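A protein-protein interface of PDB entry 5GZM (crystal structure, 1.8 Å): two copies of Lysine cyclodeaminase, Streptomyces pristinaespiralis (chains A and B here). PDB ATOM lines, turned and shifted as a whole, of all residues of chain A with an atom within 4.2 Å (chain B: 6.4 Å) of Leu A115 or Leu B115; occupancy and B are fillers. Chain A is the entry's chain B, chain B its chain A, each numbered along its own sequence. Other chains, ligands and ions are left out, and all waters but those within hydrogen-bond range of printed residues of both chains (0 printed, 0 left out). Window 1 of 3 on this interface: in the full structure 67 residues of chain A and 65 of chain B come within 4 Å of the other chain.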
ATOM      1  N   TRP A   8      -4.648 -15.452 -17.108  1.00  0.00           N
ATOM      2  CA  TRP A   8      -3.479 -16.298 -17.267  1.00  0.00           C
ATOM      3  C   TRP A   8      -2.834 -16.013 -18.614  1.00  0.00           C
ATOM      4  O   TRP A   8      -3.459 -16.182 -19.658  1.00  0.00           O
ATOM      5  CB  TRP A   8      -3.924 -17.717 -17.196  1.00  0.00           C
ATOM      6  CG  TRP A   8      -2.813 -18.763 -17.197  1.00  0.00           C
ATOM      7  CD1 TRP A   8      -1.502 -18.606 -16.866  1.00  0.00           C
ATOM      8  CD2 TRP A   8      -2.987 -20.121 -17.515  1.00  0.00           C
ATOM      9  NE1 TRP A   8      -0.853 -19.811 -16.941  1.00  0.00           N
ATOM     10  CE2 TRP A   8      -1.747 -20.756 -17.354  1.00  0.00           C
ATOM     11  CE3 TRP A   8      -4.087 -20.882 -17.885  1.00  0.00           C
ATOM     12  CZ2 TRP A   8      -1.578 -22.101 -17.583  1.00  0.00           C
ATOM     13  CZ3 TRP A   8      -3.914 -22.223 -18.105  1.00  0.00           C
ATOM     14  CH2 TRP A   8      -2.669 -22.810 -17.974  1.00  0.00           C
ATOM     15  N   VAL A   9      -1.600 -15.585 -18.550  1.00  0.00           N
ATOM     16  CA  VAL A   9      -0.889 -15.193 -19.748  1.00  0.00           C
ATOM     17  C   VAL A   9       0.257 -16.170 -20.019  1.00  0.00           C
ATOM     18  O   VAL A   9       1.079 -16.394 -19.150  1.00  0.00           O
ATOM     19  CB  VAL A   9      -0.358 -13.788 -19.600  1.00  0.00           C
ATOM     20  CG1 VAL A   9       0.407 -13.389 -20.841  1.00  0.00           C
ATOM     21  CG2 VAL A   9      -1.495 -12.817 -19.357  1.00  0.00           C
ATOM     22  N   LEU A  10       0.258 -16.764 -21.213  1.00  0.00           N
ATOM     23  CA  LEU A  10       1.358 -17.619 -21.665  1.00  0.00           C
ATOM     24  C   LEU A  10       2.179 -16.957 -22.790  1.00  0.00           C
ATOM     25  O   LEU A  10       1.705 -16.835 -23.916  1.00  0.00           O
ATOM     26  CB  LEU A  10       0.796 -18.921 -22.212  1.00  0.00           C
ATOM     27  CG  LEU A  10       0.052 -19.896 -21.296  1.00  0.00           C
ATOM     28  CD1 LEU A  10      -0.285 -21.114 -22.154  1.00  0.00           C
ATOM     29  CD2 LEU A  10       0.891 -20.282 -20.068  1.00  0.00           C
ATOM     30  N   VAL A 102      -3.891 -15.075 -29.235  1.00  0.00           N
ATOM     31  CA  VAL A 102      -5.150 -15.727 -29.038  1.00  0.00           C
ATOM     32  C   VAL A 102      -5.615 -15.538 -27.592  1.00  0.00           C
ATOM     33  O   VAL A 102      -4.870 -15.802 -26.662  1.00  0.00           O
ATOM     34  CB  VAL A 102      -5.024 -17.222 -29.291  1.00  0.00           C
ATOM     35  CG1 VAL A 102      -6.376 -17.848 -29.509  1.00  0.00           C
ATOM     36  CG2 VAL A 102      -4.130 -17.405 -30.521  1.00  0.00           C
ATOM     37  N   ALA A 103      -6.852 -15.090 -27.471  1.00  0.00           N
ATOM     38  CA  ALA A 103      -7.424 -14.726 -26.185  1.00  0.00           C
ATOM     39  C   ALA A 103      -8.636 -15.599 -25.943  1.00  0.00           C
ATOM     40  O   ALA A 103      -9.346 -15.953 -26.884  1.00  0.00           O
ATOM     41  CB  ALA A 103      -7.806 -13.255 -26.187  1.00  0.00           C
ATOM     42  N   ALA A 114      -7.754 -16.015 -20.439  1.00  0.00           N
ATOM     43  CA  ALA A 114      -6.391 -16.355 -20.861  1.00  0.00           C
ATOM     44  C   ALA A 114      -5.995 -15.668 -22.178  1.00  0.00           C
ATOM     45  O   ALA A 114      -6.851 -15.313 -22.977  1.00  0.00           O
ATOM     46  CB  ALA A 114      -6.191 -17.869 -20.968  1.00  0.00           C
ATOM     47  N   LEU A 115      -4.688 -15.482 -22.307  1.00  0.00           N
ATOM     48  CA  LEU A 115      -4.068 -14.820 -23.436  1.00  0.00           C
ATOM     49  C   LEU A 115      -2.717 -15.438 -23.729  1.00  0.00           C
ATOM     50  O   LEU A 115      -1.871 -15.516 -22.853  1.00  0.00           O
ATOM     51  CB  LEU A 115      -3.803 -13.360 -23.087  1.00  0.00           C
ATOM     52  CG  LEU A 115      -3.208 -12.460 -24.173  1.00  0.00           C
ATOM     53  CD1 LEU A 115      -4.027 -12.540 -25.430  1.00  0.00           C
ATOM     54  CD2 LEU A 115      -3.164 -11.074 -23.560  1.00  0.00           C
ATOM     55  N   MET A 116      -2.481 -15.798 -24.988  1.00  0.00           N
ATOM     56  CA  MET A 116      -1.235 -16.420 -25.326  1.00  0.00           C
ATOM     57  C   MET A 116      -0.723 -16.020 -26.712  1.00  0.00           C
ATOM     58  O   MET A 116      -1.434 -15.448 -27.518  1.00  0.00           O
ATOM     59  CB  MET A 116      -1.403 -17.949 -25.242  1.00  0.00           C
ATOM     60  CG  MET A 116      -2.224 -18.593 -26.289  1.00  0.00           C
ATOM     61  SD  MET A 116      -2.071 -20.405 -26.202  1.00  0.00           S
ATOM     62  CE  MET A 116      -0.420 -20.640 -26.839  1.00  0.00           C
ATOM     63  N   ILE A 334      -5.746  -7.923 -14.893  1.00  0.00           N
ATOM     64  CA  ILE A 334      -5.802  -6.871 -15.933  1.00  0.00           C
ATOM     65  C   ILE A 334      -7.112  -6.104 -15.714  1.00  0.00           C
ATOM     66  O   ILE A 334      -7.119  -4.903 -15.431  1.00  0.00           O
ATOM     67  CB  ILE A 334      -5.700  -7.484 -17.323  1.00  0.00           C
ATOM     68  CG1 ILE A 334      -4.322  -8.150 -17.456  1.00  0.00           C
ATOM     69  CG2 ILE A 334      -5.879  -6.428 -18.438  1.00  0.00           C
ATOM     70  CD1 ILE A 334      -4.196  -9.085 -18.629  1.00  0.00           C
ATOM     71  N   THR B   7       4.797  -6.604 -24.983  1.00  0.00           N
ATOM     72  CA  THR B   7       3.497  -5.966 -24.775  1.00  0.00           C
ATOM     73  C   THR B   7       3.506  -5.272 -23.426  1.00  0.00           C
ATOM     74  O   THR B   7       3.780  -5.875 -22.387  1.00  0.00           O
ATOM     75  CB  THR B   7       2.402  -7.004 -24.744  1.00  0.00           C
ATOM     76  OG1 THR B   7       2.419  -7.728 -25.972  1.00  0.00           O
ATOM     77  CG2 THR B   7       1.018  -6.362 -24.437  1.00  0.00           C
ATOM     78  N   TRP B   8       3.152  -4.004 -23.420  1.00  0.00           N
ATOM     79  CA  TRP B   8       3.165  -3.230 -22.182  1.00  0.00           C
ATOM     80  C   TRP B   8       1.781  -3.423 -21.595  1.00  0.00           C
ATOM     81  O   TRP B   8       0.769  -3.072 -22.212  1.00  0.00           O
ATOM     82  CB  TRP B   8       3.416  -1.761 -22.547  1.00  0.00           C
ATOM     83  CG  TRP B   8       3.499  -0.815 -21.380  1.00  0.00           C
ATOM     84  CD1 TRP B   8       3.744  -1.127 -20.072  1.00  0.00           C
ATOM     85  CD2 TRP B   8       3.356   0.608 -21.423  1.00  0.00           C
ATOM     86  NE1 TRP B   8       3.776   0.013 -19.304  1.00  0.00           N
ATOM     87  CE2 TRP B   8       3.535   1.087 -20.109  1.00  0.00           C
ATOM     88  CE3 TRP B   8       3.117   1.522 -22.458  1.00  0.00           C
ATOM     89  CZ2 TRP B   8       3.437   2.460 -19.788  1.00  0.00           C
ATOM     90  CZ3 TRP B   8       2.983   2.856 -22.153  1.00  0.00           C
ATOM     91  CH2 TRP B   8       3.182   3.322 -20.820  1.00  0.00           C
ATOM     92  N   VAL B   9       1.704  -4.044 -20.432  1.00  0.00           N
ATOM     93  CA  VAL B   9       0.425  -4.356 -19.813  1.00  0.00           C
ATOM     94  C   VAL B   9       0.178  -3.435 -18.603  1.00  0.00           C
ATOM     95  O   VAL B   9       0.976  -3.381 -17.678  1.00  0.00           O
ATOM     96  CB  VAL B   9       0.347  -5.834 -19.359  1.00  0.00           C
ATOM     97  CG1 VAL B   9      -1.026  -6.129 -18.789  1.00  0.00           C
ATOM     98  CG2 VAL B   9       0.611  -6.792 -20.522  1.00  0.00           C
ATOM     99  N   LEU B  10      -0.940  -2.756 -18.665  1.00  0.00           N
ATOM    100  CA  LEU B  10      -1.513  -2.003 -17.569  1.00  0.00           C
ATOM    101  C   LEU B  10      -2.802  -2.703 -17.129  1.00  0.00           C
ATOM    102  O   LEU B  10      -3.892  -2.570 -17.748  1.00  0.00           O
ATOM    103  CB  LEU B  10      -1.946  -0.646 -18.059  1.00  0.00           C
ATOM    104  CG  LEU B  10      -0.949   0.293 -18.724  1.00  0.00           C
ATOM    105  CD1 LEU B  10      -1.676   1.629 -18.823  1.00  0.00           C
ATOM    106  CD2 LEU B  10       0.344   0.427 -17.926  1.00  0.00           C
ATOM    107  N   GLY B  11      -2.668  -3.401 -16.064  1.00  0.00           N
ATOM    108  CA  GLY B  11      -3.810  -3.915 -15.351  1.00  0.00           C
ATOM    109  C   GLY B  11      -4.186  -3.064 -14.150  1.00  0.00           C
ATOM    110  O   GLY B  11      -3.713  -1.928 -13.947  1.00  0.00           O
ATOM    111  N   THR B 101     -11.414  -5.238 -22.212  1.00  0.00           N
ATOM    112  CA  THR B 101     -10.022  -4.835 -22.266  1.00  0.00           C
ATOM    113  C   THR B 101      -9.807  -4.083 -23.573  1.00  0.00           C
ATOM    114  O   THR B 101     -10.545  -4.264 -24.553  1.00  0.00           O
ATOM    115  CB  THR B 101      -9.102  -6.069 -22.252  1.00  0.00           C
ATOM    116  OG1 THR B 101      -9.692  -7.083 -23.039  1.00  0.00           O
ATOM    117  CG2 THR B 101      -8.901  -6.561 -20.859  1.00  0.00           C
ATOM    118  N   VAL B 102      -8.778  -3.255 -23.590  1.00  0.00           N
ATOM    119  CA  VAL B 102      -8.395  -2.549 -24.809  1.00  0.00           C
ATOM    120  C   VAL B 102      -6.933  -2.844 -25.183  1.00  0.00           C
ATOM    121  O   VAL B 102      -6.067  -2.724 -24.359  1.00  0.00           O
ATOM    122  CB  VAL B 102      -8.540  -1.032 -24.649  1.00  0.00           C
ATOM    123  CG1 VAL B 102      -8.502  -0.333 -26.001  1.00  0.00           C
ATOM    124  CG2 VAL B 102      -9.845  -0.706 -23.912  1.00  0.00           C
ATOM    125  N   ALA B 103      -6.723  -3.238 -26.415  1.00  0.00           N
ATOM    126  CA  ALA B 103      -5.430  -3.653 -26.910  1.00  0.00           C
ATOM    127  C   ALA B 103      -5.060  -2.736 -28.058  1.00  0.00           C
ATOM    128  O   ALA B 103      -5.924  -2.242 -28.794  1.00  0.00           O
ATOM    129  CB  ALA B 103      -5.497  -5.105 -27.402  1.00  0.00           C
ATOM    130  N   ARG B 104      -3.745  -2.511 -28.208  1.00  0.00           N
ATOM    131  CA  ARG B 104      -3.238  -1.775 -29.313  1.00  0.00           C
ATOM    132  C   ARG B 104      -2.205  -2.610 -30.069  1.00  0.00           C
ATOM    133  O   ARG B 104      -1.334  -3.252 -29.425  1.00  0.00           O
ATOM    134  CB  ARG B 104      -2.626  -0.495 -28.823  1.00  0.00           C
ATOM    135  CG  ARG B 104      -1.918   0.311 -29.902  1.00  0.00           C
ATOM    136  CD  ARG B 104      -1.420   1.625 -29.298  1.00  0.00           C
ATOM    137  NE  ARG B 104      -2.538   2.493 -28.889  1.00  0.00           N
ATOM    138  CZ  ARG B 104      -2.400   3.771 -28.541  1.00  0.00           C
ATOM    139  NH1 ARG B 104      -1.209   4.344 -28.556  1.00  0.00           N
ATOM    140  NH2 ARG B 104      -3.463   4.493 -28.188  1.00  0.00           N
ATOM    141  N   LEU B 112       1.318  -6.830 -31.027  1.00  0.00           N
ATOM    142  CA  LEU B 112       0.594  -6.382 -29.826  1.00  0.00           C
ATOM    143  C   LEU B 112       1.505  -5.583 -28.914  1.00  0.00           C
ATOM    144  O   LEU B 112       2.416  -6.128 -28.314  1.00  0.00           O
ATOM    145  CB  LEU B 112       0.018  -7.576 -29.093  1.00  0.00           C
ATOM    146  CG  LEU B 112      -0.688  -7.283 -27.787  1.00  0.00           C
ATOM    147  CD1 LEU B 112      -1.923  -6.459 -27.975  1.00  0.00           C
ATOM    148  CD2 LEU B 112      -1.005  -8.523 -27.012  1.00  0.00           C
ATOM    149  N   THR B 113       1.272  -4.262 -28.840  1.00  0.00           N
ATOM    150  CA  THR B 113       2.180  -3.359 -28.100  1.00  0.00           C
ATOM    151  C   THR B 113       1.715  -2.972 -26.734  1.00  0.00           C
ATOM    152  O   THR B 113       2.499  -2.634 -25.874  1.00  0.00           O
ATOM    153  CB  THR B 113       2.486  -2.073 -28.907  1.00  0.00           C
ATOM    154  OG1 THR B 113       1.265  -1.435 -29.250  1.00  0.00           O
ATOM    155  CG2 THR B 113       3.256  -2.394 -30.161  1.00  0.00           C
ATOM    156  N   ALA B 114       0.418  -3.021 -26.494  1.00  0.00           N
ATOM    157  CA  ALA B 114      -0.114  -2.629 -25.188  1.00  0.00           C
ATOM    158  C   ALA B 114      -1.511  -3.226 -24.980  1.00  0.00           C
ATOM    159  O   ALA B 114      -2.236  -3.460 -25.941  1.00  0.00           O
ATOM    160  CB  ALA B 114      -0.192  -1.128 -25.108  1.00  0.00           C
ATOM    161  N   LEU B 115      -1.827  -3.432 -23.711  1.00  0.00           N
ATOM    162  CA  LEU B 115      -3.048  -4.047 -23.276  1.00  0.00           C
ATOM    163  C   LEU B 115      -3.428  -3.519 -21.900  1.00  0.00           C
ATOM    164  O   LEU B 115      -2.596  -3.428 -20.986  1.00  0.00           O
ATOM    165  CB  LEU B 115      -2.872  -5.578 -23.251  1.00  0.00           C
ATOM    166  CG  LEU B 115      -4.078  -6.354 -22.648  1.00  0.00           C
ATOM    167  CD1 LEU B 115      -5.269  -6.219 -23.554  1.00  0.00           C
ATOM    168  CD2 LEU B 115      -3.771  -7.838 -22.450  1.00  0.00           C
ATOM    169  N   MET B 116      -4.688  -3.107 -21.747  1.00  0.00           N
ATOM    170  CA  MET B 116      -5.139  -2.588 -20.485  1.00  0.00           C
ATOM    171  C   MET B 116      -6.594  -2.889 -20.204  1.00  0.00           C
ATOM    172  O   MET B 116      -7.324  -3.266 -21.084  1.00  0.00           O
ATOM    173  CB  MET B 116      -4.912  -1.061 -20.383  1.00  0.00           C
ATOM    174  CG  MET B 116      -5.579  -0.256 -21.494  1.00  0.00           C
ATOM    175  SD  MET B 116      -5.506   1.519 -21.204  1.00  0.00           S
ATOM    176  CE  MET B 116      -6.166   1.724 -19.542  1.00  0.00           C
ATOM    177  N   ASP B 117      -6.954  -2.754 -18.942  1.00  0.00           N
ATOM    178  CA  ASP B 117      -8.345  -2.828 -18.462  1.00  0.00           C
ATOM    179  C   ASP B 117      -9.216  -1.906 -19.302  1.00  0.00           C
ATOM    180  O   ASP B 117      -8.804  -0.779 -19.621  1.00  0.00           O
ATOM    181  CB  ASP B 117      -8.403  -2.301 -17.046  1.00  0.00           C
ATOM    182  CG  ASP B 117      -9.839  -2.086 -16.572  1.00  0.00           C
ATOM    183  OD1 ASP B 117     -10.601  -3.084 -16.634  1.00  0.00           O
ATOM    184  OD2 ASP B 117     -10.195  -0.946 -16.168  1.00  0.00           O
ATOM    185  N   MET B 316      -7.298   5.604 -24.186  1.00  0.00           N
ATOM    186  CA  MET B 316      -6.158   4.768 -23.921  1.00  0.00           C
ATOM    187  C   MET B 316      -4.848   5.567 -23.993  1.00  0.00           C
ATOM    188  O   MET B 316      -3.960   5.351 -23.157  1.00  0.00           O
ATOM    189  CB  MET B 316      -6.156   3.534 -24.865  1.00  0.00           C
ATOM    190  CG  MET B 316      -4.957   2.608 -24.698  1.00  0.00           C
ATOM    191  SD  MET B 316      -5.262   0.954 -25.351  1.00  0.00           S
ATOM    192  CE  MET B 316      -3.695   0.149 -24.993  1.00  0.00           C
ATOM    193  N   LEU B 320      -1.903   5.731 -21.343  1.00  0.00           N
ATOM    194  CA  LEU B 320      -0.517   5.385 -21.692  1.00  0.00           C
ATOM    195  C   LEU B 320       0.467   6.508 -21.415  1.00  0.00           C
ATOM    196  O   LEU B 320       1.589   6.266 -20.931  1.00  0.00           O
ATOM    197  CB  LEU B 320      -0.361   4.893 -23.123  1.00  0.00           C
ATOM    198  CG  LEU B 320      -1.178   3.668 -23.501  1.00  0.00           C
ATOM    199  CD1 LEU B 320      -0.964   3.381 -24.972  1.00  0.00           C
ATOM    200  CD2 LEU B 320      -0.819   2.489 -22.629  1.00  0.00           C
ATOM    201  N   ILE B 334       4.699 -11.623 -24.988  1.00  0.00           N
ATOM    202  CA  ILE B 334       3.559 -12.502 -25.238  1.00  0.00           C
ATOM    203  C   ILE B 334       3.703 -13.236 -26.576  1.00  0.00           C
ATOM    204  O   ILE B 334       3.758 -14.469 -26.630  1.00  0.00           O
ATOM    205  CB  ILE B 334       2.220 -11.755 -25.134  1.00  0.00           C
ATOM    206  CG1 ILE B 334       2.127 -11.109 -23.726  1.00  0.00           C
ATOM    207  CG2 ILE B 334       1.061 -12.740 -25.402  1.00  0.00           C
ATOM    208  CD1 ILE B 334       0.864 -10.274 -23.505  1.00  0.00           C
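N of Leu B115 sits at hydrogen-bond distance from O of Trp B8, 3.0 Å away. N of Leu B10 lies within hydrogen-bond range of O of Leu B115, 2.9 Å away. The backbone carbonyl oxygen (O) of Leu B10 lies within hydrogen-bond range of the backbone NH (N) of Asp B117 (3.3 Å). O of Trp A8 sits at hydrogen-bond distance from N of Leu A115, 3.0 Å away. The backbone NH of Leu A10 is in hydrogen-bond range of the backbone carbonyl oxygen of Leu A115 (3.0 Å). O of Val A102 lies within hydrogen-bond range of N of Met A116, 2.9 Å away.
Among the printed residues, pairs that only touch across the chains: Ile A334 with Asp B117 (3.3 Å), Ile A334 with Gly B11 (3.5 Å), Leu A115 with Leu B115 (3.5 Å), Ile A334 with Thr B101 (3.9 Å) and Met A116 with Ile B334 (3.96 Å).
Leu A115 touches just one residue of chain B: Leu B115. Leu B115 touches just one residue of chain A: Leu A115 (3.5 Å). Of the printed residues of chain A, Asp B117 touches Ile A334. Printed residues of chain B within 4 Å of Ile A334: Gly B11, Thr B101 and Asp B117. Of the printed residues of chain A, Thr B101 touches Ile A334. The nearest residue of chain B that does not touch Leu A115 is Ile B334 (4.1 Å). The nearest printed residue of chain A that does not touch Thr B101 is Ala A103 (7.2 Å).
Of the 18 printed residues of chain B, 5 touch a printed residue of chain A. Printed residues of chain B that touch a printed residue of chain A: Gly B11, Thr B101, Leu B115, Asp B117 and Ile B334. Printed residues of chain A that touch a printed residue of chain B: Leu A115, Met A116 and Ile A334. Among the printed residues, 5 pairs touch across the chains.
Leu A115 touches its own counterpart, Leu B115. Met A116 touches Ile B334, but with the chains exchanged Ile A334 does not touch Met B116 (4.02 Å).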
